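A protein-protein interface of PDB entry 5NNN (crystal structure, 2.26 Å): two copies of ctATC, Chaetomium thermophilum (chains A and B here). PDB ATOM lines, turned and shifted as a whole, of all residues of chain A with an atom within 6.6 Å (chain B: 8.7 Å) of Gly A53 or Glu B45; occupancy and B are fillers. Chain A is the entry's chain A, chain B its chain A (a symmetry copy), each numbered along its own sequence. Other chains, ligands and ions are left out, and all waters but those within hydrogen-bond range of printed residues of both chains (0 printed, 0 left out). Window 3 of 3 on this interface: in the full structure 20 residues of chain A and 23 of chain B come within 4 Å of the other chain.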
ATOM      1  N   LEU A  51      -1.516 -24.051 -14.946  1.00  0.00           N
ATOM      2  CA  LEU A  51      -1.299 -24.744 -16.218  1.00  0.00           C
ATOM      3  C   LEU A  51      -0.182 -24.144 -17.072  1.00  0.00           C
ATOM      4  O   LEU A  51      -0.164 -24.360 -18.301  1.00  0.00           O
ATOM      5  CB  LEU A  51      -2.598 -24.813 -17.026  1.00  0.00           C
ATOM      6  CG  LEU A  51      -3.756 -25.644 -16.469  1.00  0.00           C
ATOM      7  CD1 LEU A  51      -4.893 -25.752 -17.531  1.00  0.00           C
ATOM      8  CD2 LEU A  51      -3.290 -27.049 -16.040  1.00  0.00           C
ATOM      9  N   ARG A  52       0.808 -23.471 -16.464  1.00  0.00           N
ATOM     10  CA  ARG A  52       2.068 -23.243 -17.185  1.00  0.00           C
ATOM     11  C   ARG A  52       2.508 -24.544 -17.844  1.00  0.00           C
ATOM     12  O   ARG A  52       2.361 -25.631 -17.279  1.00  0.00           O
ATOM     13  CB  ARG A  52       3.176 -22.732 -16.265  1.00  0.00           C
ATOM     14  CG  ARG A  52       2.986 -21.296 -15.784  1.00  0.00           C
ATOM     15  CD  ARG A  52       4.292 -20.647 -15.271  1.00  0.00           C
ATOM     16  NE  ARG A  52       5.266 -20.364 -16.329  1.00  0.00           N
ATOM     17  CZ  ARG A  52       5.255 -19.286 -17.121  1.00  0.00           C
ATOM     18  NH1 ARG A  52       4.306 -18.354 -17.018  1.00  0.00           N
ATOM     19  NH2 ARG A  52       6.201 -19.141 -18.043  1.00  0.00           N
ATOM     20  N   GLY A  53       2.993 -24.449 -19.064  1.00  0.00           N
ATOM     21  CA  GLY A  53       3.396 -25.643 -19.790  1.00  0.00           C
ATOM     22  C   GLY A  53       2.287 -26.364 -20.533  1.00  0.00           C
ATOM     23  O   GLY A  53       2.565 -27.365 -21.214  1.00  0.00           O
ATOM     24  N   LYS A  54       1.039 -25.923 -20.404  1.00  0.00           N
ATOM     25  CA  LYS A  54      -0.060 -26.519 -21.146  1.00  0.00           C
ATOM     26  C   LYS A  54      -0.542 -25.574 -22.250  1.00  0.00           C
ATOM     27  O   LYS A  54      -0.604 -24.354 -22.068  1.00  0.00           O
ATOM     28  CB  LYS A  54      -1.209 -26.888 -20.197  1.00  0.00           C
ATOM     29  CG  LYS A  54      -0.795 -27.906 -19.092  1.00  0.00           C
ATOM     30  CD  LYS A  54      -0.438 -29.265 -19.692  1.00  0.00           C
ATOM     31  CE  LYS A  54       0.063 -30.249 -18.634  1.00  0.00           C
ATOM     32  NZ  LYS A  54       0.573 -31.510 -19.251  1.00  0.00           N
ATOM     33  N   VAL A  55      -0.916 -26.158 -23.382  1.00  0.00           N
ATOM     34  CA  VAL A  55      -1.386 -25.423 -24.549  1.00  0.00           C
ATOM     35  C   VAL A  55      -2.807 -25.882 -24.867  1.00  0.00           C
ATOM     36  O   VAL A  55      -3.051 -27.084 -25.045  1.00  0.00           O
ATOM     37  CB  VAL A  55      -0.462 -25.648 -25.757  1.00  0.00           C
ATOM     38  CG1 VAL A  55      -0.985 -24.877 -26.987  1.00  0.00           C
ATOM     39  CG2 VAL A  55       1.004 -25.295 -25.394  1.00  0.00           C
ATOM     40  N   MET A  75      -8.004 -20.221 -20.053  1.00  0.00           N
ATOM     41  CA  MET A  75      -6.700 -20.863 -20.157  1.00  0.00           C
ATOM     42  C   MET A  75      -5.589 -19.906 -19.751  1.00  0.00           C
ATOM     43  O   MET A  75      -4.696 -20.264 -18.961  1.00  0.00           O
ATOM     44  CB  MET A  75      -6.430 -21.381 -21.550  1.00  0.00           C
ATOM     45  CG  MET A  75      -5.138 -22.138 -21.570  1.00  0.00           C
ATOM     46  SD  MET A  75      -5.358 -23.696 -20.653  1.00  0.00           S
ATOM     47  CE  MET A  75      -3.883 -24.529 -21.199  1.00  0.00           C
ATOM     48  N   GLY A  79      -2.469 -19.556 -16.488  1.00  0.00           N
ATOM     49  CA  GLY A  79      -1.081 -19.552 -16.870  1.00  0.00           C
ATOM     50  C   GLY A  79      -0.729 -20.434 -18.043  1.00  0.00           C
ATOM     51  O   GLY A  79       0.457 -20.530 -18.383  1.00  0.00           O
ATOM     52  N   GLY A  80      -1.706 -21.074 -18.687  1.00  0.00           N
ATOM     53  CA  GLY A  80      -1.437 -21.784 -19.919  1.00  0.00           C
ATOM     54  C   GLY A  80      -1.337 -20.868 -21.143  1.00  0.00           C
ATOM     55  O   GLY A  80      -1.475 -19.647 -21.070  1.00  0.00           O
ATOM     56  N   ARG A  81      -1.069 -21.501 -22.288  1.00  0.00           N
ATOM     57  CA  ARG A  81      -0.992 -20.847 -23.586  1.00  0.00           C
ATOM     58  C   ARG A  81      -2.157 -21.310 -24.454  1.00  0.00           C
ATOM     59  O   ARG A  81      -2.602 -22.461 -24.357  1.00  0.00           O
ATOM     60  CB  ARG A  81       0.312 -21.181 -24.300  1.00  0.00           C
ATOM     61  CG  ARG A  81       1.611 -20.858 -23.555  1.00  0.00           C
ATOM     62  CD  ARG A  81       1.693 -19.400 -23.131  1.00  0.00           C
ATOM     63  NE  ARG A  81       3.070 -18.982 -22.883  1.00  0.00           N
ATOM     64  CZ  ARG A  81       3.885 -18.447 -23.799  1.00  0.00           C
ATOM     65  NH1 ARG A  81       3.467 -18.249 -25.054  1.00  0.00           N
ATOM     66  NH2 ARG A  81       5.132 -18.098 -23.466  1.00  0.00           N
ATOM     67  N   ASP A 110      -2.468 -29.631 -25.887  1.00  0.00           N
ATOM     68  CA  ASP A 110      -2.851 -30.649 -24.925  1.00  0.00           C
ATOM     69  C   ASP A 110      -4.357 -30.834 -24.834  1.00  0.00           C
ATOM     70  O   ASP A 110      -4.808 -31.813 -24.263  1.00  0.00           O
ATOM     71  CB  ASP A 110      -2.236 -30.273 -23.563  1.00  0.00           C
ATOM     72  CG  ASP A 110      -0.722 -30.022 -23.677  1.00  0.00           C
ATOM     73  OD1 ASP A 110      -0.013 -30.879 -24.269  1.00  0.00           O
ATOM     74  OD2 ASP A 110      -0.244 -28.951 -23.261  1.00  0.00           O
ATOM     75  N   LEU B   2      21.333 -28.552 -24.669  1.00  0.00           N
ATOM     76  CA  LEU B   2      20.554 -27.792 -25.634  1.00  0.00           C
ATOM     77  C   LEU B   2      21.055 -26.357 -25.707  1.00  0.00           C
ATOM     78  O   LEU B   2      21.255 -25.820 -26.798  1.00  0.00           O
ATOM     79  CB  LEU B   2      19.073 -27.835 -25.248  1.00  0.00           C
ATOM     80  CG  LEU B   2      18.043 -27.142 -26.144  1.00  0.00           C
ATOM     81  CD1 LEU B   2      18.264 -27.492 -27.616  1.00  0.00           C
ATOM     82  CD2 LEU B   2      16.628 -27.537 -25.705  1.00  0.00           C
ATOM     83  N   GLU B  37      16.312 -32.661 -29.185  1.00  0.00           N
ATOM     84  CA  GLU B  37      16.330 -32.070 -27.849  1.00  0.00           C
ATOM     85  C   GLU B  37      15.016 -31.355 -27.536  1.00  0.00           C
ATOM     86  O   GLU B  37      14.486 -31.452 -26.417  1.00  0.00           O
ATOM     87  CB  GLU B  37      17.518 -31.113 -27.720  1.00  0.00           C
ATOM     88  CG  GLU B  37      18.813 -31.773 -27.219  1.00  0.00           C
ATOM     89  CD  GLU B  37      18.687 -32.391 -25.834  1.00  0.00           C
ATOM     90  OE1 GLU B  37      18.958 -31.677 -24.839  1.00  0.00           O
ATOM     91  OE2 GLU B  37      18.323 -33.586 -25.737  1.00  0.00           O
ATOM     92  N   MET B  38      14.475 -30.622 -28.507  1.00  0.00           N
ATOM     93  CA  MET B  38      13.204 -29.947 -28.291  1.00  0.00           C
ATOM     94  C   MET B  38      12.144 -30.953 -27.876  1.00  0.00           C
ATOM     95  O   MET B  38      11.397 -30.727 -26.916  1.00  0.00           O
ATOM     96  CB  MET B  38      12.794 -29.180 -29.562  1.00  0.00           C
ATOM     97  CG  MET B  38      13.602 -27.917 -29.801  1.00  0.00           C
ATOM     98  SD  MET B  38      13.614 -26.830 -28.379  1.00  0.00           S
ATOM     99  CE  MET B  38      14.611 -25.526 -29.021  1.00  0.00           C
ATOM    100  N   ARG B  39      12.091 -32.105 -28.554  1.00  0.00           N
ATOM    101  CA  ARG B  39      11.079 -33.099 -28.184  1.00  0.00           C
ATOM    102  C   ARG B  39      11.252 -33.550 -26.743  1.00  0.00           C
ATOM    103  O   ARG B  39      10.257 -33.810 -26.046  1.00  0.00           O
ATOM    104  CB  ARG B  39      11.110 -34.309 -29.117  1.00  0.00           C
ATOM    105  CG  ARG B  39      10.206 -35.445 -28.632  1.00  0.00           C
ATOM    106  CD  ARG B  39      10.197 -36.593 -29.569  1.00  0.00           C
ATOM    107  NE  ARG B  39      11.513 -36.739 -30.153  1.00  0.00           N
ATOM    108  CZ  ARG B  39      11.773 -37.386 -31.284  1.00  0.00           C
ATOM    109  NH1 ARG B  39      10.792 -37.957 -31.974  1.00  0.00           N
ATOM    110  NH2 ARG B  39      13.024 -37.446 -31.724  1.00  0.00           N
ATOM    111  N   LEU B  40      12.506 -33.640 -26.269  1.00  0.00           N
ATOM    112  CA  LEU B  40      12.702 -34.081 -24.882  1.00  0.00           C
ATOM    113  C   LEU B  40      12.271 -32.997 -23.902  1.00  0.00           C
ATOM    114  O   LEU B  40      11.496 -33.255 -22.961  1.00  0.00           O
ATOM    115  CB  LEU B  40      14.165 -34.464 -24.636  1.00  0.00           C
ATOM    116  CG  LEU B  40      14.794 -35.618 -25.431  1.00  0.00           C
ATOM    117  CD1 LEU B  40      16.237 -35.682 -25.041  1.00  0.00           C
ATOM    118  CD2 LEU B  40      14.144 -36.950 -25.188  1.00  0.00           C
ATOM    119  N   GLY B  41      12.769 -31.777 -24.112  1.00  0.00           N
ATOM    120  CA  GLY B  41      12.362 -30.665 -23.267  1.00  0.00           C
ATOM    121  C   GLY B  41      10.855 -30.578 -23.139  1.00  0.00           C
ATOM    122  O   GLY B  41      10.314 -30.490 -22.037  1.00  0.00           O
ATOM    123  N   VAL B  42      10.147 -30.630 -24.273  1.00  0.00           N
ATOM    124  CA  VAL B  42       8.699 -30.497 -24.219  1.00  0.00           C
ATOM    125  C   VAL B  42       8.081 -31.684 -23.515  1.00  0.00           C
ATOM    126  O   VAL B  42       7.087 -31.538 -22.802  1.00  0.00           O
ATOM    127  CB  VAL B  42       8.112 -30.329 -25.633  1.00  0.00           C
ATOM    128  CG1 VAL B  42       6.618 -30.597 -25.628  1.00  0.00           C
ATOM    129  CG2 VAL B  42       8.395 -28.942 -26.144  1.00  0.00           C
ATOM    130  N   GLN B  43       8.601 -32.891 -23.758  1.00  0.00           N
ATOM    131  CA  GLN B  43       7.993 -34.048 -23.108  1.00  0.00           C
ATOM    132  C   GLN B  43       8.045 -33.917 -21.597  1.00  0.00           C
ATOM    133  O   GLN B  43       7.130 -34.384 -20.905  1.00  0.00           O
ATOM    134  CB  GLN B  43       8.659 -35.332 -23.576  1.00  0.00           C
ATOM    135  CG  GLN B  43       7.757 -36.123 -24.552  1.00  0.00           C
ATOM    136  CD  GLN B  43       8.539 -37.028 -25.500  1.00  0.00           C
ATOM    137  OE1 GLN B  43       9.770 -37.062 -25.462  1.00  0.00           O
ATOM    138  NE2 GLN B  43       7.818 -37.749 -26.377  1.00  0.00           N
ATOM    139  N   ARG B  44       9.044 -33.211 -21.069  1.00  0.00           N
ATOM    140  CA  ARG B  44       9.121 -33.071 -19.621  1.00  0.00           C
ATOM    141  C   ARG B  44       8.508 -31.795 -19.065  1.00  0.00           C
ATOM    142  O   ARG B  44       7.991 -31.843 -17.947  1.00  0.00           O
ATOM    143  CB  ARG B  44      10.581 -33.186 -19.139  1.00  0.00           C
ATOM    144  CG  ARG B  44      11.544 -32.167 -19.677  1.00  0.00           C
ATOM    145  CD  ARG B  44      12.910 -32.266 -18.977  1.00  0.00           C
ATOM    146  NE  ARG B  44      13.967 -31.648 -19.787  1.00  0.00           N
ATOM    147  CZ  ARG B  44      14.761 -32.305 -20.635  1.00  0.00           C
ATOM    148  NH1 ARG B  44      14.649 -33.621 -20.788  1.00  0.00           N
ATOM    149  NH2 ARG B  44      15.678 -31.643 -21.331  1.00  0.00           N
ATOM    150  N   GLU B  45       8.532 -30.646 -19.778  1.00  0.00           N
ATOM    151  CA  GLU B  45       8.025 -29.400 -19.190  1.00  0.00           C
ATOM    152  C   GLU B  45       7.019 -28.589 -20.012  1.00  0.00           C
ATOM    153  O   GLU B  45       6.562 -27.549 -19.511  1.00  0.00           O
ATOM    154  CB  GLU B  45       9.178 -28.462 -18.810  1.00  0.00           C
ATOM    155  CG  GLU B  45      10.381 -28.458 -19.706  1.00  0.00           C
ATOM    156  CD  GLU B  45      11.527 -27.650 -19.102  1.00  0.00           C
ATOM    157  OE1 GLU B  45      11.255 -26.551 -18.561  1.00  0.00           O
ATOM    158  OE2 GLU B  45      12.686 -28.116 -19.158  1.00  0.00           O
ATOM    159  N   GLY B  46       6.645 -29.022 -21.228  1.00  0.00           N
ATOM    160  CA  GLY B  46       5.547 -28.399 -21.962  1.00  0.00           C
ATOM    161  C   GLY B  46       5.921 -27.097 -22.641  1.00  0.00           C
ATOM    162  O   GLY B  46       6.047 -27.046 -23.870  1.00  0.00           O
ATOM    163  N   VAL B  47       6.133 -26.050 -21.848  1.00  0.00           N
ATOM    164  CA  VAL B  47       6.629 -24.766 -22.326  1.00  0.00           C
ATOM    165  C   VAL B  47       8.028 -24.549 -21.748  1.00  0.00           C
ATOM    166  O   VAL B  47       8.188 -24.409 -20.527  1.00  0.00           O
ATOM    167  CB  VAL B  47       5.686 -23.631 -21.913  1.00  0.00           C
ATOM    168  CG1 VAL B  47       6.298 -22.289 -22.243  1.00  0.00           C
ATOM    169  CG2 VAL B  47       4.315 -23.812 -22.541  1.00  0.00           C
ATOM    170  N   LEU B  48       9.029 -24.485 -22.632  1.00  0.00           N
ATOM    171  CA  LEU B  48      10.421 -24.196 -22.283  1.00  0.00           C
ATOM    172  C   LEU B  48      10.707 -22.708 -22.070  1.00  0.00           C
ATOM    173  O   LEU B  48       9.787 -21.891 -21.907  1.00  0.00           O
ATOM    174  CB  LEU B  48      11.382 -24.708 -23.371  1.00  0.00           C
ATOM    175  CG  LEU B  48      11.184 -26.109 -23.958  1.00  0.00           C
ATOM    176  CD1 LEU B  48      12.376 -26.521 -24.845  1.00  0.00           C
ATOM    177  CD2 LEU B  48      10.947 -27.108 -22.868  1.00  0.00           C
ATOM    178  N   ASP B  49      12.011 -22.364 -22.116  1.00  0.00           N
ATOM    179  CA  ASP B  49      12.565 -21.078 -21.698  1.00  0.00           C
ATOM    180  C   ASP B  49      13.392 -20.380 -22.771  1.00  0.00           C
ATOM    181  O   ASP B  49      13.805 -19.226 -22.571  1.00  0.00           O
ATOM    182  CB  ASP B  49      13.481 -21.293 -20.487  1.00  0.00           C
ATOM    183  CG  ASP B  49      13.349 -20.224 -19.474  1.00  0.00           C
ATOM    184  OD1 ASP B  49      12.578 -19.277 -19.726  1.00  0.00           O
ATOM    185  OD2 ASP B  49      13.999 -20.351 -18.419  1.00  0.00           O
ATOM    186  N   ILE B  50      13.644 -21.051 -23.893  1.00  0.00           N
ATOM    187  CA  ILE B  50      14.615 -20.607 -24.892  1.00  0.00           C
ATOM    188  C   ILE B  50      14.355 -19.181 -25.352  1.00  0.00           C
ATOM    189  O   ILE B  50      15.296 -18.392 -25.514  1.00  0.00           O
ATOM    190  CB  ILE B  50      14.605 -21.568 -26.097  1.00  0.00           C
ATOM    191  CG1 ILE B  50      14.502 -23.035 -25.652  1.00  0.00           C
ATOM    192  CG2 ILE B  50      15.811 -21.307 -27.009  1.00  0.00           C
ATOM    193  CD1 ILE B  50      15.388 -23.418 -24.533  1.00  0.00           C
ATOM    194  N   GLN B  76       5.324 -20.568 -28.918  1.00  0.00           N
ATOM    195  CA  GLN B  76       4.872 -20.458 -27.538  1.00  0.00           C
ATOM    196  C   GLN B  76       5.517 -21.534 -26.661  1.00  0.00           C
ATOM    197  O   GLN B  76       5.751 -21.315 -25.466  1.00  0.00           O
ATOM    198  CB  GLN B  76       3.338 -20.539 -27.461  1.00  0.00           C
ATOM    199  CG  GLN B  76       2.662 -19.282 -28.025  1.00  0.00           C
ATOM    200  CD  GLN B  76       1.229 -19.099 -27.626  1.00  0.00           C
ATOM    201  OE1 GLN B  76       0.928 -18.770 -26.470  1.00  0.00           O
ATOM    202  NE2 GLN B  76       0.321 -19.238 -28.604  1.00  0.00           N
ATOM    203  N   ARG B  77       5.785 -22.700 -27.221  1.00  0.00           N
ATOM    204  CA  ARG B  77       6.407 -23.743 -26.437  1.00  0.00           C
ATOM    205  C   ARG B  77       7.895 -23.481 -26.215  1.00  0.00           C
ATOM    206  O   ARG B  77       8.473 -24.081 -25.313  1.00  0.00           O
ATOM    207  CB  ARG B  77       6.184 -25.087 -27.103  1.00  0.00           C
ATOM    208  CG  ARG B  77       4.833 -25.737 -26.775  1.00  0.00           C
ATOM    209  CD  ARG B  77       4.786 -27.127 -27.358  1.00  0.00           C
ATOM    210  NE  ARG B  77       3.464 -27.780 -27.345  1.00  0.00           N
ATOM    211  CZ  ARG B  77       2.830 -28.180 -26.244  1.00  0.00           C
ATOM    212  NH1 ARG B  77       3.355 -27.970 -25.055  1.00  0.00           N
ATOM    213  NH2 ARG B  77       1.662 -28.782 -26.331  1.00  0.00           N
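The side-chain amide oxygen (OE1) of Gln B76 lies within hydrogen-bond range of the guanidinium group (NH1) of Arg A81, 3.0 Å away. The guanidinium group of Arg B77 is in salt-bridge range of the side-chain carboxylate of Asp A110, at 3.4 Å.
The backbone carbonyl oxygen of Lys A54 is in hydrogen-bond range of the backbone NH of Arg A81 (2.9 Å). The backbone carbonyl oxygen of Val A55 is in hydrogen-bond range of the backbone NH of Asp A110 (2.7 Å). OE2 of Glu B45 is in salt-bridge range of NE of Arg B44 (3.8 Å). NH1 of Arg B77 is in hydrogen-bond range of O of Gly B46 (3.1 Å). The backbone NH (N) of Leu B48 lies within hydrogen-bond range of the backbone carbonyl oxygen (O) of Arg B77 (2.8 Å).
Glu B45 touches Gly A53 (O to CA, 3.7 Å). CA of Gly B46 touches O of Gly A53, at 3.2 Å. Gly A53 touches Val B47. Arg B77 touches Gly A53 (NH1 to O, 3.97 Å). Val A55 touches Arg B77.
Gly A53 touches just these residues of chain B: Glu B45 (3.7 Å), Gly B46 (3.2 Å), Val B47 (3.4 Å) and Arg B77 (3.97 Å). Glu B45 touches one residue of chain A. Of the printed residues of chain B, Arg A81 touches Gln B76. Printed residues of chain A within 4 Å of Gly B46: Gly A53 (3.2 Å). Of the printed residues of chain A, Gln B76 touches Arg A81 (3.0 Å). The nearest residue of chain A that does not touch Glu B45 is Arg A52 (5.1 Å). The nearest printed residue of chain A that does not touch Gln B76 is Val A55 (5.7 Å).
Of the 10 printed residues of chain A, 4 touch a printed residue of chain B. Hydrophobic or aromatic side chains of chain A that line the printed part of chain B: Val A55. Along chain A the printed residues that touch a printed residue of chain B span positions 53 to 110. Of the 17 printed residues of chain B, 5 touch a printed residue of chain A. Printed residues of chain B that touch a printed residue of chain A: Glu B45, Gly B46, Val B47, Gln B76 and Arg B77. Hydrophobic or aromatic side chains of chain B within 4 Å of the printed part of chain A: Val B47.
No position is printed for both chains. Of the 7 pairs that touch across the chains among the printed residues, none has its exchanged pair printed and touching as well.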
